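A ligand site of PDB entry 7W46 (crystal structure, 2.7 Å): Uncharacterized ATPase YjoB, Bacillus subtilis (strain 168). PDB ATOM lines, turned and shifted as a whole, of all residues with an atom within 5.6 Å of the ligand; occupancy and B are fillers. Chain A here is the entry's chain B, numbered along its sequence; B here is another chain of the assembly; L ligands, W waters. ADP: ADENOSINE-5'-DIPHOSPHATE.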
ATOM      1  N   GLN A 188      24.368  21.158  33.798  1.00  0.00           N
ATOM      2  CA  GLN A 188      24.009  21.066  32.388  1.00  0.00           C
ATOM      3  C   GLN A 188      23.069  22.193  31.952  1.00  0.00           C
ATOM      4  O   GLN A 188      22.549  22.141  30.819  1.00  0.00           O
ATOM      5  CB  GLN A 188      23.341  19.730  32.074  1.00  0.00           C
ATOM      6  CG  GLN A 188      23.779  18.537  32.893  1.00  0.00           C
ATOM      7  CD  GLN A 188      23.043  17.282  32.482  1.00  0.00           C
ATOM      8  OE1 GLN A 188      22.097  16.813  33.151  1.00  0.00           O
ATOM      9  NE2 GLN A 188      23.459  16.713  31.357  1.00  0.00           N
ATOM     10  N   VAL A 189      22.804  23.163  32.819  1.00  0.00           N
ATOM     11  CA  VAL A 189      21.978  24.309  32.482  1.00  0.00           C
ATOM     12  C   VAL A 189      22.936  25.420  32.038  1.00  0.00           C
ATOM     13  O   VAL A 189      23.558  26.097  32.870  1.00  0.00           O
ATOM     14  CB  VAL A 189      21.102  24.724  33.664  1.00  0.00           C
ATOM     15  CG1 VAL A 189      20.288  25.966  33.326  1.00  0.00           C
ATOM     16  CG2 VAL A 189      20.185  23.597  34.029  1.00  0.00           C
ATOM     17  N   ILE A 190      23.062  25.619  30.728  1.00  0.00           N
ATOM     18  CA  ILE A 190      24.045  26.553  30.187  1.00  0.00           C
ATOM     19  C   ILE A 190      23.478  27.967  30.174  1.00  0.00           C
ATOM     20  O   ILE A 190      22.466  28.248  29.515  1.00  0.00           O
ATOM     21  CB  ILE A 190      24.481  26.135  28.779  1.00  0.00           C
ATOM     22  CG1 ILE A 190      24.861  24.648  28.780  1.00  0.00           C
ATOM     23  CG2 ILE A 190      25.609  27.074  28.328  1.00  0.00           C
ATOM     24  CD1 ILE A 190      25.861  24.252  29.850  1.00  0.00           C
ATOM     25  N   MET A 191      24.165  28.873  30.858  1.00  0.00           N
ATOM     26  CA  MET A 191      23.543  30.135  31.164  1.00  0.00           C
ATOM     27  C   MET A 191      24.638  31.079  31.654  1.00  0.00           C
ATOM     28  O   MET A 191      25.712  30.644  32.098  1.00  0.00           O
ATOM     29  CB  MET A 191      22.444  29.932  32.204  1.00  0.00           C
ATOM     30  CG  MET A 191      21.595  31.135  32.502  1.00  0.00           C
ATOM     31  SD  MET A 191      19.965  30.579  33.041  1.00  0.00           S
ATOM     32  CE  MET A 191      19.462  29.543  31.634  1.00  0.00           C
ATOM     33  N   PRO A 230      12.968  34.337  24.460  1.00  0.00           N
ATOM     34  CA  PRO A 230      12.737  33.595  23.204  1.00  0.00           C
ATOM     35  C   PRO A 230      12.774  32.092  23.443  1.00  0.00           C
ATOM     36  O   PRO A 230      13.613  31.588  24.209  1.00  0.00           O
ATOM     37  CB  PRO A 230      13.903  34.052  22.308  1.00  0.00           C
ATOM     38  CG  PRO A 230      14.915  34.680  23.248  1.00  0.00           C
ATOM     39  CD  PRO A 230      14.120  35.241  24.388  1.00  0.00           C
ATOM     40  N   PRO A 231      11.883  31.342  22.802  1.00  0.00           N
ATOM     41  CA  PRO A 231      11.750  29.912  23.125  1.00  0.00           C
ATOM     42  C   PRO A 231      12.990  29.112  22.735  1.00  0.00           C
ATOM     43  O   PRO A 231      13.785  29.496  21.873  1.00  0.00           O
ATOM     44  CB  PRO A 231      10.541  29.467  22.286  1.00  0.00           C
ATOM     45  CG  PRO A 231      10.443  30.469  21.200  1.00  0.00           C
ATOM     46  CD  PRO A 231      10.957  31.771  21.742  1.00  0.00           C
ATOM     47  N   GLY A 232      13.137  27.980  23.417  1.00  0.00           N
ATOM     48  CA  GLY A 232      14.224  27.045  23.161  1.00  0.00           C
ATOM     49  C   GLY A 232      15.540  27.382  23.837  1.00  0.00           C
ATOM     50  O   GLY A 232      16.582  26.897  23.394  1.00  0.00           O
ATOM     51  N   ASN A 233      15.527  28.196  24.902  1.00  0.00           N
ATOM     52  CA  ASN A 233      16.776  28.680  25.468  1.00  0.00           C
ATOM     53  C   ASN A 233      16.929  28.423  26.951  1.00  0.00           C
ATOM     54  O   ASN A 233      17.925  28.857  27.528  1.00  0.00           O
ATOM     55  CB  ASN A 233      16.946  30.165  25.170  1.00  0.00           C
ATOM     56  CG  ASN A 233      17.121  30.425  23.715  1.00  0.00           C
ATOM     57  OD1 ASN A 233      18.133  30.030  23.134  1.00  0.00           O
ATOM     58  ND2 ASN A 233      16.112  31.013  23.085  1.00  0.00           N
ATOM     59  N   GLY A 234      16.000  27.722  27.583  1.00  0.00           N
ATOM     60  CA  GLY A 234      16.323  27.093  28.839  1.00  0.00           C
ATOM     61  C   GLY A 234      15.372  27.310  29.992  1.00  0.00           C
ATOM     62  O   GLY A 234      15.716  26.986  31.137  1.00  0.00           O
ATOM     63  N   LYS A 235      14.182  27.844  29.728  1.00  0.00           N
ATOM     64  CA  LYS A 235      13.206  28.012  30.799  1.00  0.00           C
ATOM     65  C   LYS A 235      12.814  26.664  31.395  1.00  0.00           C
ATOM     66  O   LYS A 235      13.003  26.418  32.598  1.00  0.00           O
ATOM     67  CB  LYS A 235      11.977  28.744  30.258  1.00  0.00           C
ATOM     68  CG  LYS A 235      12.214  30.192  29.826  1.00  0.00           C
ATOM     69  CD  LYS A 235      10.939  30.768  29.239  1.00  0.00           C
ATOM     70  CE  LYS A 235      11.195  31.498  27.956  1.00  0.00           C
ATOM     71  NZ  LYS A 235      11.704  30.619  26.878  1.00  0.00           N
ATOM     72  N   THR A 236      12.255  25.768  30.565  1.00  0.00           N
ATOM     73  CA  THR A 236      11.936  24.419  31.030  1.00  0.00           C
ATOM     74  C   THR A 236      13.164  23.722  31.584  1.00  0.00           C
ATOM     75  O   THR A 236      13.089  23.026  32.598  1.00  0.00           O
ATOM     76  CB  THR A 236      11.336  23.579  29.881  1.00  0.00           C
ATOM     77  OG1 THR A 236      10.195  24.228  29.314  1.00  0.00           O
ATOM     78  CG2 THR A 236      10.911  22.238  30.399  1.00  0.00           C
ATOM     79  N   THR A 237      14.324  23.889  30.922  1.00  0.00           N
ATOM     80  CA  THR A 237      15.527  23.210  31.362  1.00  0.00           C
ATOM     81  C   THR A 237      15.904  23.657  32.768  1.00  0.00           C
ATOM     82  O   THR A 237      16.204  22.819  33.637  1.00  0.00           O
ATOM     83  CB  THR A 237      16.667  23.453  30.363  1.00  0.00           C
ATOM     84  OG1 THR A 237      16.357  22.805  29.117  1.00  0.00           O
ATOM     85  CG2 THR A 237      18.032  22.933  30.856  1.00  0.00           C
ATOM     86  N   LEU A 238      15.871  24.972  33.021  1.00  0.00           N
ATOM     87  CA  LEU A 238      16.151  25.480  34.360  1.00  0.00           C
ATOM     88  C   LEU A 238      15.178  24.925  35.385  1.00  0.00           C
ATOM     89  O   LEU A 238      15.566  24.560  36.507  1.00  0.00           O
ATOM     90  CB  LEU A 238      16.096  27.008  34.366  1.00  0.00           C
ATOM     91  CG  LEU A 238      16.617  27.623  35.663  1.00  0.00           C
ATOM     92  CD1 LEU A 238      18.119  27.553  35.686  1.00  0.00           C
ATOM     93  CD2 LEU A 238      16.180  29.058  35.777  1.00  0.00           C
ATOM     94  N   LYS A 240      13.380  22.064  35.251  1.00  0.00           N
ATOM     95  CA  LYS A 240      13.695  20.658  35.486  1.00  0.00           C
ATOM     96  C   LYS A 240      14.895  20.486  36.407  1.00  0.00           C
ATOM     97  O   LYS A 240      14.890  19.616  37.292  1.00  0.00           O
ATOM     98  CB  LYS A 240      13.947  19.952  34.160  1.00  0.00           C
ATOM     99  CG  LYS A 240      12.688  19.711  33.359  1.00  0.00           C
ATOM    100  CD  LYS A 240      12.983  19.395  31.906  1.00  0.00           C
ATOM    101  CE  LYS A 240      13.222  17.910  31.719  1.00  0.00           C
ATOM    102  NZ  LYS A 240      13.720  17.594  30.342  1.00  0.00           N
ATOM    103  N   THR A 313       6.639  30.875  33.917  1.00  0.00           N
ATOM    104  CA  THR A 313       7.402  30.694  32.695  1.00  0.00           C
ATOM    105  C   THR A 313       6.569  31.209  31.548  1.00  0.00           C
ATOM    106  O   THR A 313       5.381  30.934  31.476  1.00  0.00           O
ATOM    107  CB  THR A 313       7.762  29.207  32.524  1.00  0.00           C
ATOM    108  OG1 THR A 313       8.908  28.911  33.331  1.00  0.00           O
ATOM    109  CG2 THR A 313       7.968  28.810  31.078  1.00  0.00           C
ATOM    110  N   ASN A 315       6.846  32.309  27.134  1.00  0.00           N
ATOM    111  CA  ASN A 315       7.444  32.693  25.871  1.00  0.00           C
ATOM    112  C   ASN A 315       6.794  33.934  25.298  1.00  0.00           C
ATOM    113  O   ASN A 315       7.290  34.499  24.305  1.00  0.00           O
ATOM    114  CB  ASN A 315       7.342  31.532  24.886  1.00  0.00           C
ATOM    115  CG  ASN A 315       8.325  30.441  25.213  1.00  0.00           C
ATOM    116  OD1 ASN A 315       9.519  30.698  25.370  1.00  0.00           O
ATOM    117  ND2 ASN A 315       7.836  29.216  25.323  1.00  0.00           N
ATOM    118  N   TYR A 348      27.957  24.846  25.575  1.00  0.00           N
ATOM    119  CA  TYR A 348      26.885  23.889  25.350  1.00  0.00           C
ATOM    120  C   TYR A 348      27.373  22.716  24.529  1.00  0.00           C
ATOM    121  O   TYR A 348      27.112  21.551  24.867  1.00  0.00           O
ATOM    122  CB  TYR A 348      25.699  24.545  24.646  1.00  0.00           C
ATOM    123  CG  TYR A 348      24.610  23.550  24.286  1.00  0.00           C
ATOM    124  CD1 TYR A 348      23.600  23.249  25.188  1.00  0.00           C
ATOM    125  CD2 TYR A 348      24.590  22.908  23.053  1.00  0.00           C
ATOM    126  CE1 TYR A 348      22.612  22.355  24.875  1.00  0.00           C
ATOM    127  CE2 TYR A 348      23.598  21.984  22.733  1.00  0.00           C
ATOM    128  CZ  TYR A 348      22.611  21.722  23.647  1.00  0.00           C
ATOM    129  OH  TYR A 348      21.630  20.820  23.362  1.00  0.00           O
ATOM    130  N   MET A 351      29.498  20.192  26.688  1.00  0.00           N
ATOM    131  CA  MET A 351      28.795  19.323  27.634  1.00  0.00           C
ATOM    132  C   MET A 351      27.817  18.412  26.920  1.00  0.00           C
ATOM    133  O   MET A 351      27.525  17.319  27.403  1.00  0.00           O
ATOM    134  CB  MET A 351      28.109  20.150  28.719  1.00  0.00           C
ATOM    135  CG  MET A 351      26.786  20.698  28.324  1.00  0.00           C
ATOM    136  SD  MET A 351      25.363  19.706  28.834  1.00  0.00           S
ATOM    137  CE  MET A 351      24.191  20.184  27.587  1.00  0.00           C
ATOM    138  N   ARG A 352      27.331  18.829  25.753  1.00  0.00           N
ATOM    139  CA  ARG A 352      26.353  18.018  25.056  1.00  0.00           C
ATOM    140  C   ARG A 352      26.963  16.768  24.433  1.00  0.00           C
ATOM    141  O   ARG A 352      26.229  15.821  24.143  1.00  0.00           O
ATOM    142  CB  ARG A 352      25.658  18.854  23.982  1.00  0.00           C
ATOM    143  CG  ARG A 352      24.382  18.248  23.445  1.00  0.00           C
ATOM    144  CD  ARG A 352      23.332  18.108  24.526  1.00  0.00           C
ATOM    145  NE  ARG A 352      22.168  17.422  23.979  1.00  0.00           N
ATOM    146  CZ  ARG A 352      22.041  16.102  23.937  1.00  0.00           C
ATOM    147  NH1 ARG A 352      23.020  15.339  24.426  1.00  0.00           N
ATOM    148  NH2 ARG A 352      20.965  15.544  23.415  1.00  0.00           N
ATOM    149  N   PHE A 375      19.708  27.290  21.941  1.00  0.00           N
ATOM    150  CA  PHE A 375      20.216  26.021  22.463  1.00  0.00           C
ATOM    151  C   PHE A 375      19.445  24.850  21.868  1.00  0.00           C
ATOM    152  O   PHE A 375      20.042  23.850  21.456  1.00  0.00           O
ATOM    153  CB  PHE A 375      20.143  26.003  23.989  1.00  0.00           C
ATOM    154  CG  PHE A 375      21.139  26.904  24.679  1.00  0.00           C
ATOM    155  CD1 PHE A 375      22.501  26.668  24.562  1.00  0.00           C
ATOM    156  CD2 PHE A 375      20.708  27.951  25.472  1.00  0.00           C
ATOM    157  CE1 PHE A 375      23.419  27.485  25.223  1.00  0.00           C
ATOM    158  CE2 PHE A 375      21.626  28.768  26.133  1.00  0.00           C
ATOM    159  CZ  PHE A 375      22.977  28.523  26.016  1.00  0.00           C
ATOM    160  N   ALA A 376      18.118  24.975  21.803  1.00  0.00           N
ATOM    161  CA  ALA A 376      17.312  23.881  21.266  1.00  0.00           C
ATOM    162  C   ALA A 376      17.696  23.535  19.830  1.00  0.00           C
ATOM    163  O   ALA A 376      17.616  22.377  19.423  1.00  0.00           O
ATOM    164  CB  ALA A 376      15.816  24.212  21.349  1.00  0.00           C
ATOM    165  N   ASP B 300       6.880  18.950  24.868  1.00  0.00           N
ATOM    166  CA  ASP B 300       8.196  19.397  25.301  1.00  0.00           C
ATOM    167  C   ASP B 300       8.208  20.073  26.670  1.00  0.00           C
ATOM    168  O   ASP B 300       9.259  20.583  27.092  1.00  0.00           O
ATOM    169  CB  ASP B 300       8.780  20.341  24.226  1.00  0.00           C
ATOM    170  CG  ASP B 300      10.312  20.468  24.277  1.00  0.00           C
ATOM    171  OD1 ASP B 300      10.983  19.600  24.910  1.00  0.00           O
ATOM    172  OD2 ASP B 300      10.838  21.444  23.676  1.00  0.00           O
ATOM    173  N   ARG B 330       8.848  23.613  18.334  1.00  0.00           N
ATOM    174  CA  ARG B 330       8.631  22.625  19.386  1.00  0.00           C
ATOM    175  C   ARG B 330       8.378  21.208  18.853  1.00  0.00           C
ATOM    176  O   ARG B 330       8.364  20.249  19.641  1.00  0.00           O
ATOM    177  CB  ARG B 330       7.447  23.064  20.280  1.00  0.00           C
ATOM    178  CG  ARG B 330       7.516  24.546  20.659  1.00  0.00           C
ATOM    179  CD  ARG B 330       6.892  24.792  22.004  1.00  0.00           C
ATOM    180  NE  ARG B 330       7.311  23.767  22.950  1.00  0.00           N
ATOM    181  CZ  ARG B 330       6.829  23.664  24.181  1.00  0.00           C
ATOM    182  NH1 ARG B 330       5.919  24.532  24.603  1.00  0.00           N
ATOM    183  NH2 ARG B 330       7.270  22.710  24.984  1.00  0.00           N
HETATM  184  PB  ADP L   1      12.201  26.941  26.706  1.00  0.00           P
HETATM  185  O1B ADP L   1      11.417  26.248  27.817  1.00  0.00           O
HETATM  186  O2B ADP L   1      12.914  28.180  27.193  1.00  0.00           O
HETATM  187  O3B ADP L   1      11.512  27.147  25.377  1.00  0.00           O
HETATM  188  PA  ADP L   1      13.629  24.427  26.883  1.00  0.00           P
HETATM  189  O1A ADP L   1      12.291  23.735  26.739  1.00  0.00           O
HETATM  190  O2A ADP L   1      14.386  24.449  28.192  1.00  0.00           O
HETATM  191  O3A ADP L   1      13.423  25.941  26.364  1.00  0.00           O
HETATM  192  O5' ADP L   1      14.642  23.870  25.795  1.00  0.00           O
HETATM  193  C5' ADP L   1      14.284  22.918  24.796  1.00  0.00           C
HETATM  194  C4' ADP L   1      15.441  21.944  24.661  1.00  0.00           C
HETATM  195  O4' ADP L   1      16.637  22.602  24.180  1.00  0.00           O
HETATM  196  C3' ADP L   1      15.779  21.397  26.025  1.00  0.00           C
HETATM  197  O3' ADP L   1      15.108  20.160  26.272  1.00  0.00           O
HETATM  198  C2' ADP L   1      17.282  21.236  25.992  1.00  0.00           C
HETATM  199  O2' ADP L   1      17.565  19.970  25.415  1.00  0.00           O
HETATM  200  C1' ADP L   1      17.756  22.292  25.011  1.00  0.00           C
HETATM  201  N9  ADP L   1      18.126  23.505  25.792  1.00  0.00           N
HETATM  202  C8  ADP L   1      17.514  24.694  25.689  1.00  0.00           C
HETATM  203  N7  ADP L   1      18.058  25.610  26.520  1.00  0.00           N
HETATM  204  C5  ADP L   1      19.055  25.002  27.190  1.00  0.00           C
HETATM  205  C6  ADP L   1      20.031  25.411  28.213  1.00  0.00           C
HETATM  206  N6  ADP L   1      20.027  26.682  28.671  1.00  0.00           N
HETATM  207  N1  ADP L   1      20.919  24.490  28.670  1.00  0.00           N
HETATM  208  C2  ADP L   1      20.913  23.219  28.189  1.00  0.00           C
HETATM  209  N3  ADP L   1      20.041  22.787  27.252  1.00  0.00           N
HETATM  210  C4  ADP L   1      19.098  23.618  26.712  1.00  0.00           C
HETATM  211  O   HOH W   1      20.476  19.896  25.407  1.00  0.00           O
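An oxygen (O3B) of the ligand lies within hydrogen-bond range of the backbone NH (N) of Gly 232 (2.7 Å).
N of Thr 237 is in hydrogen-bond range of O2A of the ligand, 2.8 Å away.
The side-chain hydroxyl (OG1) of Thr 237 is in hydrogen-bond range of an oxygen (O2A) of the ligand (2.7 Å).
An oxygen (O2B) of the ligand sits at hydrogen-bond distance from the backbone NH of Lys 235.
An oxygen (O2B) of the ligand is in salt-bridge range of the side-chain amino group of Lys 235 (2.7 Å).
The backbone NH (N) of Thr 236 is in hydrogen-bond range of an oxygen (O1B) of the ligand (2.9 Å).
The side-chain hydroxyl (OG1) of Thr 236 is in hydrogen-bond range of an oxygen (O1B) of the ligand, at 2.8 Å.
N of Ile 190 sits at hydrogen-bond distance from N1 of the ligand, 3.2 Å away.
N6 of the ligand lies within hydrogen-bond range of O of Ile 190.
The backbone NH of Asn 233 lies within hydrogen-bond range of an oxygen (O3A) of the ligand, at 3.4 Å.
The backbone carbonyl oxygen (O) of Asn 233 is in hydrogen-bond range of a nitrogen (N6) of the ligand.
The backbone NH of Gly 234 lies within hydrogen-bond range of a nitrogen (N7) of the ligand, at 3.1 Å.
O of Gly 232 sits at hydrogen-bond distance from N of Ala 376.
The backbone NH of Phe 375 lies within hydrogen-bond range of the backbone carbonyl oxygen of Gly 232.
The side-chain amino group (NZ) of Lys 235 sits at hydrogen-bond distance from the side-chain amide oxygen (OD1) of Asn 315, at 2.7 Å.
The backbone carbonyl oxygen (O) of Pro 230 is in hydrogen-bond range of the side-chain amino group (NZ) of Lys 235.
The side-chain amide oxygen (OD1) of Asn 233 is in hydrogen-bond range of the backbone NH (N) of Phe 375, at 3.4 Å.
The backbone carbonyl oxygen (O) of Pro 231 lies within hydrogen-bond range of the side-chain amide nitrogen (ND2) of Asn 233, 3.0 Å away.
The side-chain amide nitrogen (ND2) of Asn 233 is in hydrogen-bond range of the backbone carbonyl oxygen (O) of Pro 230.
The side-chain hydroxyl of Tyr 348 lies close to the guanidinium group of Arg 352, 3.5 Å away.
Merely in contact with the ligand: Ala 376, Gln 188, Phe 375, Tyr 348, Pro 231, Asp 300 of chain B and Val 189.
Hydrophobic or aromatic side chains within 4 Å of the ligand: Ile 190, Pro 231, Tyr 348, Phe 375 and Ala 376.
14 residues have an atom within 4 Å of the ligand: Gln 188, Val 189, Ile 190, Pro 231, Gly 232, Asn 233, Gly 234, Lys 235, Thr 236, Thr 237, Tyr 348, Phe 375, Ala 376 and Asp 300 of chain B.
The nearest printed residue that does not touch the ligand is Asn 315 (4.1 Å).
Water W1 lies within hydrogen-bond range of OH of Tyr 348 (2.5 Å), O2' of the ligand (2.9 Å) and NE of Arg 352 (3.3 Å).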
